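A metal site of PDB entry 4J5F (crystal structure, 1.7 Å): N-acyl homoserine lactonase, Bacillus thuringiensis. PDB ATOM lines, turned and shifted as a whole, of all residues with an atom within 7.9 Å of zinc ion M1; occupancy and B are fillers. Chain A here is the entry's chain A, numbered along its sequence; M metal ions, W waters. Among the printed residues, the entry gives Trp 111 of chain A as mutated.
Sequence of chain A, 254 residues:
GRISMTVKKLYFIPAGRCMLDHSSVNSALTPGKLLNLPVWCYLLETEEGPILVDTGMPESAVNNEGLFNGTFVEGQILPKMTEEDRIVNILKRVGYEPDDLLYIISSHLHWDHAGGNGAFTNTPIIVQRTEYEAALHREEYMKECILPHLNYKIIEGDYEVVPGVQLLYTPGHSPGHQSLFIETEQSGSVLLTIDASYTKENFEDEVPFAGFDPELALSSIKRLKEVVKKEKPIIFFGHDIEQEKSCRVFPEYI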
ATOM      1  N   SER A 107      20.494  25.702   9.019  1.00  0.00           N
ATOM      2  CA  SER A 107      21.593  26.677   9.175  1.00  0.00           C
ATOM      3  C   SER A 107      21.124  28.023   8.667  1.00  0.00           C
ATOM      4  O   SER A 107      21.390  29.070   9.279  1.00  0.00           O
ATOM      5  CB  SER A 107      22.791  26.239   8.345  1.00  0.00           C
ATOM      6  OG  SER A 107      22.409  26.078   6.985  1.00  0.00           O
ATOM      7  N   HIS A 108      20.461  27.985   7.509  1.00  0.00           N
ATOM      8  CA  HIS A 108      19.751  29.133   6.963  1.00  0.00           C
ATOM      9  C   HIS A 108      18.772  28.667   5.885  1.00  0.00           C
ATOM     10  O   HIS A 108      18.687  27.468   5.622  1.00  0.00           O
ATOM     11  CB  HIS A 108      20.715  30.158   6.397  1.00  0.00           C
ATOM     12  CG  HIS A 108      21.639  29.638   5.338  1.00  0.00           C
ATOM     13  ND1 HIS A 108      22.431  28.513   5.511  1.00  0.00           N
ATOM     14  CD2 HIS A 108      21.977  30.149   4.132  1.00  0.00           C
ATOM     15  CE1 HIS A 108      23.194  28.349   4.448  1.00  0.00           C
ATOM     16  NE2 HIS A 108      22.942  29.317   3.589  1.00  0.00           N
ATOM     17  N   LEU A 109      17.998  29.583   5.300  1.00  0.00           N
ATOM     18  CA  LEU A 109      16.932  29.180   4.414  1.00  0.00           C
ATOM     19  C   LEU A 109      17.228  29.383   2.909  1.00  0.00           C
ATOM     20  O   LEU A 109      16.286  29.430   2.084  1.00  0.00           O
ATOM     21  CB  LEU A 109      15.631  29.923   4.815  1.00  0.00           C
ATOM     22  CG  LEU A 109      15.192  29.528   6.248  1.00  0.00           C
ATOM     23  CD1 LEU A 109      13.897  30.359   6.596  1.00  0.00           C
ATOM     24  CD2 LEU A 109      14.913  28.026   6.395  1.00  0.00           C
ATOM     25  N   HIS A 110      18.503  29.476   2.539  1.00  0.00           N
ATOM     26  CA  HIS A 110      18.871  29.505   1.123  1.00  0.00           C
ATOM     27  C   HIS A 110      18.401  28.215   0.457  1.00  0.00           C
ATOM     28  O   HIS A 110      18.251  27.189   1.111  1.00  0.00           O
ATOM     29  CB  HIS A 110      20.371  29.643   0.917  1.00  0.00           C
ATOM     30  CG  HIS A 110      20.895  31.030   1.120  1.00  0.00           C
ATOM     31  ND1 HIS A 110      22.251  31.287   1.265  1.00  0.00           N
ATOM     32  CD2 HIS A 110      20.273  32.239   1.211  1.00  0.00           C
ATOM     33  CE1 HIS A 110      22.436  32.593   1.421  1.00  0.00           C
ATOM     34  NE2 HIS A 110      21.255  33.186   1.413  1.00  0.00           N
ATOM     35  N   TRP A 111      18.187  28.293  -0.862  1.00  0.00           N
ATOM     36  CA  TRP A 111      17.583  27.222  -1.665  1.00  0.00           C
ATOM     37  C   TRP A 111      18.335  25.862  -1.546  1.00  0.00           C
ATOM     38  O   TRP A 111      17.710  24.807  -1.674  1.00  0.00           O
ATOM     39  CB  TRP A 111      17.501  27.696  -3.143  1.00  0.00           C
ATOM     40  CG  TRP A 111      18.852  27.611  -3.767  1.00  0.00           C
ATOM     41  CD1 TRP A 111      19.899  28.488  -3.614  1.00  0.00           C
ATOM     42  CD2 TRP A 111      19.326  26.557  -4.601  1.00  0.00           C
ATOM     43  NE1 TRP A 111      21.000  28.029  -4.319  1.00  0.00           N
ATOM     44  CE2 TRP A 111      20.670  26.845  -4.930  1.00  0.00           C
ATOM     45  CE3 TRP A 111      18.742  25.398  -5.123  1.00  0.00           C
ATOM     46  CZ2 TRP A 111      21.439  26.006  -5.747  1.00  0.00           C
ATOM     47  CZ3 TRP A 111      19.503  24.565  -5.939  1.00  0.00           C
ATOM     48  CH2 TRP A 111      20.841  24.869  -6.230  1.00  0.00           C
ATOM     49  N   ASP A 112      19.624  25.906  -1.245  1.00  0.00           N
ATOM     50  CA  ASP A 112      20.436  24.673  -1.243  1.00  0.00           C
ATOM     51  C   ASP A 112      20.540  24.071   0.183  1.00  0.00           C
ATOM     52  O   ASP A 112      21.229  23.064   0.391  1.00  0.00           O
ATOM     53  CB  ASP A 112      21.842  24.901  -1.853  1.00  0.00           C
ATOM     54  CG  ASP A 112      22.612  26.034  -1.167  1.00  0.00           C
ATOM     55  OD1 ASP A 112      22.003  27.132  -0.940  1.00  0.00           O
ATOM     56  OD2 ASP A 112      23.831  25.888  -0.856  1.00  0.00           O
ATOM     57  N   HIS A 113      19.821  24.675   1.141  1.00  0.00           N
ATOM     58  CA  HIS A 113      19.867  24.250   2.549  1.00  0.00           C
ATOM     59  C   HIS A 113      18.491  23.957   3.121  1.00  0.00           C
ATOM     60  O   HIS A 113      18.371  23.208   4.086  1.00  0.00           O
ATOM     61  CB  HIS A 113      20.555  25.353   3.407  1.00  0.00           C
ATOM     62  CG  HIS A 113      21.989  25.568   3.029  1.00  0.00           C
ATOM     63  ND1 HIS A 113      23.033  24.910   3.652  1.00  0.00           N
ATOM     64  CD2 HIS A 113      22.552  26.301   2.037  1.00  0.00           C
ATOM     65  CE1 HIS A 113      24.173  25.239   3.055  1.00  0.00           C
ATOM     66  NE2 HIS A 113      23.906  26.071   2.066  1.00  0.00           N
ATOM     67  N   GLU A 131      16.671  35.074  10.251  1.00  0.00           N
ATOM     68  CA  GLU A 131      16.646  34.370   8.967  1.00  0.00           C
ATOM     69  C   GLU A 131      15.202  34.210   8.504  1.00  0.00           C
ATOM     70  O   GLU A 131      14.886  34.456   7.353  1.00  0.00           O
ATOM     71  CB  GLU A 131      17.310  32.984   9.123  1.00  0.00           C
ATOM     72  CG  GLU A 131      17.398  32.200   7.802  1.00  0.00           C
ATOM     73  CD  GLU A 131      18.393  32.855   6.826  1.00  0.00           C
ATOM     74  OE1 GLU A 131      19.242  33.678   7.276  1.00  0.00           O
ATOM     75  OE2 GLU A 131      18.373  32.486   5.633  1.00  0.00           O
ATOM     76  N   TYR A 141      15.072  34.155  -1.635  1.00  0.00           N
ATOM     77  CA  TYR A 141      14.387  33.002  -1.008  1.00  0.00           C
ATOM     78  C   TYR A 141      13.257  32.410  -1.850  1.00  0.00           C
ATOM     79  O   TYR A 141      12.315  33.101  -2.239  1.00  0.00           O
ATOM     80  CB  TYR A 141      13.852  33.388   0.361  1.00  0.00           C
ATOM     81  CG  TYR A 141      15.005  33.682   1.301  1.00  0.00           C
ATOM     82  CD1 TYR A 141      15.416  34.990   1.537  1.00  0.00           C
ATOM     83  CD2 TYR A 141      15.699  32.663   1.921  1.00  0.00           C
ATOM     84  CE1 TYR A 141      16.487  35.270   2.408  1.00  0.00           C
ATOM     85  CE2 TYR A 141      16.762  32.924   2.769  1.00  0.00           C
ATOM     86  CZ  TYR A 141      17.136  34.236   3.014  1.00  0.00           C
ATOM     87  OH  TYR A 141      18.225  34.451   3.869  1.00  0.00           O
ATOM     88  N   HIS A 173      26.591  35.837   5.793  1.00  0.00           N
ATOM     89  CA  HIS A 173      26.339  35.185   4.523  1.00  0.00           C
ATOM     90  C   HIS A 173      24.845  35.293   4.216  1.00  0.00           C
ATOM     91  O   HIS A 173      24.451  35.449   3.038  1.00  0.00           O
ATOM     92  CB  HIS A 173      26.745  33.712   4.576  1.00  0.00           C
ATOM     93  CG  HIS A 173      26.213  32.891   3.443  1.00  0.00           C
ATOM     94  ND1 HIS A 173      26.694  32.998   2.158  1.00  0.00           N
ATOM     95  CD2 HIS A 173      25.256  31.937   3.418  1.00  0.00           C
ATOM     96  CE1 HIS A 173      26.048  32.156   1.379  1.00  0.00           C
ATOM     97  NE2 HIS A 173      25.189  31.483   2.118  1.00  0.00           N
ATOM     98  N   SER A 174      24.017  35.105   5.254  1.00  0.00           N
ATOM     99  CA  SER A 174      22.574  35.424   5.184  1.00  0.00           C
ATOM    100  C   SER A 174      22.217  36.166   6.480  1.00  0.00           C
ATOM    101  O   SER A 174      23.027  36.163   7.432  1.00  0.00           O
ATOM    102  CB  SER A 174      21.689  34.183   4.998  1.00  0.00           C
ATOM    103  OG  SER A 174      21.730  33.333   6.162  1.00  0.00           O
ATOM    104  N   HIS A 177      22.097  33.440   9.486  1.00  0.00           N
ATOM    105  CA  HIS A 177      22.895  32.229   9.363  1.00  0.00           C
ATOM    106  C   HIS A 177      23.427  31.748  10.722  1.00  0.00           C
ATOM    107  O   HIS A 177      23.770  32.562  11.615  1.00  0.00           O
ATOM    108  CB  HIS A 177      24.061  32.485   8.435  1.00  0.00           C
ATOM    109  CG  HIS A 177      24.869  31.253   8.166  1.00  0.00           C
ATOM    110  ND1 HIS A 177      25.858  30.812   9.032  1.00  0.00           N
ATOM    111  CD2 HIS A 177      24.795  30.329   7.180  1.00  0.00           C
ATOM    112  CE1 HIS A 177      26.388  29.708   8.553  1.00  0.00           C
ATOM    113  NE2 HIS A 177      25.767  29.389   7.430  1.00  0.00           N
ATOM    114  N   ILE A 194      29.230  25.693   8.211  1.00  0.00           N
ATOM    115  CA  ILE A 194      28.241  25.819   7.171  1.00  0.00           C
ATOM    116  C   ILE A 194      28.704  26.950   6.283  1.00  0.00           C
ATOM    117  O   ILE A 194      29.851  27.005   5.959  1.00  0.00           O
ATOM    118  CB  ILE A 194      26.831  26.008   7.683  1.00  0.00           C
ATOM    119  CG1 ILE A 194      26.567  25.137   8.905  1.00  0.00           C
ATOM    120  CG2 ILE A 194      25.838  25.705   6.590  1.00  0.00           C
ATOM    121  CD1 ILE A 194      26.527  23.665   8.656  1.00  0.00           C
ATOM    122  N   ASP A 195      27.819  27.879   5.949  1.00  0.00           N
ATOM    123  CA  ASP A 195      28.178  28.920   4.970  1.00  0.00           C
ATOM    124  C   ASP A 195      28.759  30.203   5.586  1.00  0.00           C
ATOM    125  O   ASP A 195      28.871  31.238   4.914  1.00  0.00           O
ATOM    126  CB  ASP A 195      27.004  29.201   4.017  1.00  0.00           C
ATOM    127  CG  ASP A 195      26.745  28.072   3.023  1.00  0.00           C
ATOM    128  OD1 ASP A 195      27.460  27.029   3.097  1.00  0.00           O
ATOM    129  OD2 ASP A 195      25.807  28.186   2.171  1.00  0.00           O
ATOM    130  N   ALA A 196      29.131  30.151   6.871  1.00  0.00           N
ATOM    131  CA  ALA A 196      29.848  31.242   7.483  1.00  0.00           C
ATOM    132  C   ALA A 196      31.285  31.270   6.882  1.00  0.00           C
ATOM    133  O   ALA A 196      32.000  32.278   6.985  1.00  0.00           O
ATOM    134  CB  ALA A 196      29.849  31.122   9.024  1.00  0.00           C
ATOM    135  N   TYR A 198      32.492  29.389   2.972  1.00  0.00           N
ATOM    136  CA  TYR A 198      32.404  28.374   1.925  1.00  0.00           C
ATOM    137  C   TYR A 198      33.617  27.443   1.898  1.00  0.00           C
ATOM    138  O   TYR A 198      33.468  26.231   1.745  1.00  0.00           O
ATOM    139  CB  TYR A 198      32.313  28.971   0.519  1.00  0.00           C
ATOM    140  CG  TYR A 198      30.932  29.393   0.073  1.00  0.00           C
ATOM    141  CD1 TYR A 198      29.948  29.673   0.999  1.00  0.00           C
ATOM    142  CD2 TYR A 198      30.618  29.500  -1.258  1.00  0.00           C
ATOM    143  CE1 TYR A 198      28.682  30.079   0.587  1.00  0.00           C
ATOM    144  CE2 TYR A 198      29.357  29.912  -1.677  1.00  0.00           C
ATOM    145  CZ  TYR A 198      28.410  30.185  -0.747  1.00  0.00           C
ATOM    146  OH  TYR A 198      27.169  30.578  -1.183  1.00  0.00           O
ATOM    147  N   PHE A 209      33.455  36.329   0.218  1.00  0.00           N
ATOM    148  CA  PHE A 209      32.737  35.361  -0.601  1.00  0.00           C
ATOM    149  C   PHE A 209      31.250  35.769  -0.608  1.00  0.00           C
ATOM    150  O   PHE A 209      30.864  36.760   0.035  1.00  0.00           O
ATOM    151  CB  PHE A 209      32.911  33.936  -0.065  1.00  0.00           C
ATOM    152  CG  PHE A 209      32.306  33.717   1.292  1.00  0.00           C
ATOM    153  CD1 PHE A 209      31.112  33.024   1.441  1.00  0.00           C
ATOM    154  CD2 PHE A 209      32.925  34.236   2.426  1.00  0.00           C
ATOM    155  CE1 PHE A 209      30.550  32.848   2.715  1.00  0.00           C
ATOM    156  CE2 PHE A 209      32.371  34.072   3.687  1.00  0.00           C
ATOM    157  CZ  PHE A 209      31.192  33.365   3.833  1.00  0.00           C
ATOM    158  N   ALA A 210      30.448  34.987  -1.334  1.00  0.00           N
ATOM    159  CA  ALA A 210      29.036  35.297  -1.571  1.00  0.00           C
ATOM    160  C   ALA A 210      28.306  35.520  -0.253  1.00  0.00           C
ATOM    161  O   ALA A 210      28.413  34.681   0.666  1.00  0.00           O
ATOM    162  CB  ALA A 210      28.389  34.149  -2.352  1.00  0.00           C
ATOM    163  N   GLY A 211      27.544  36.598  -0.148  1.00  0.00           N
ATOM    164  CA  GLY A 211      26.875  36.895   1.111  1.00  0.00           C
ATOM    165  C   GLY A 211      26.004  38.127   1.098  1.00  0.00           C
ATOM    166  O   GLY A 211      26.129  38.992   0.241  1.00  0.00           O
ATOM    167  N   HIS A 239      31.183  24.693   1.468  1.00  0.00           N
ATOM    168  CA  HIS A 239      31.095  24.396   0.053  1.00  0.00           C
ATOM    169  C   HIS A 239      32.527  24.297  -0.514  1.00  0.00           C
ATOM    170  O   HIS A 239      32.919  25.089  -1.374  1.00  0.00           O
ATOM    171  CB  HIS A 239      30.270  25.499  -0.657  1.00  0.00           C
ATOM    172  CG  HIS A 239      28.771  25.455  -0.397  1.00  0.00           C
ATOM    173  ND1 HIS A 239      27.990  24.381  -0.754  1.00  0.00           N
ATOM    174  CD2 HIS A 239      27.910  26.386   0.110  1.00  0.00           C
ATOM    175  CE1 HIS A 239      26.719  24.627  -0.471  1.00  0.00           C
ATOM    176  NE2 HIS A 239      26.640  25.842   0.038  1.00  0.00           N
HETATM  177 ZN    ZN M   1      23.843  30.031   1.747  1.00  0.00          ZN
HETATM  178 ZN    ZN M   2      25.106  26.959   0.806  1.00  0.00          ZN
HETATM  179  O   HOH W   1      25.389  29.081  -0.421  1.00  0.00           O
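ND1 of His 173 lies within hydrogen-bond range of O of Ala 210 (2.8 Å).
A ring nitrogen (ND1) of His 108 sits at hydrogen-bond distance from the side-chain hydroxyl of Ser 107 (2.8 Å).
N of Asp 195 sits at hydrogen-bond distance from NE2 of His 177, at 2.9 Å.
Residues that only touch zinc ion M1: His 113 (3.96 Å).
Five residues have an atom within 4 Å of zinc ion M1: His 108, His 110, His 113, His 173 and Asp 195.
Zinc ion M1 is bound by a ring nitrogen (NE2) of His 173 (2.0 Å), a ring nitrogen (ND1) of His 110 (2.1 Å) and a ring nitrogen (NE2) of His 108 (2.2 Å).
Slightly farther from zinc ion M1 lies OD2 of Asp 195 (2.7 Å).
Slightly farther from zinc ion M1 lies water W1 (2.8 Å).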
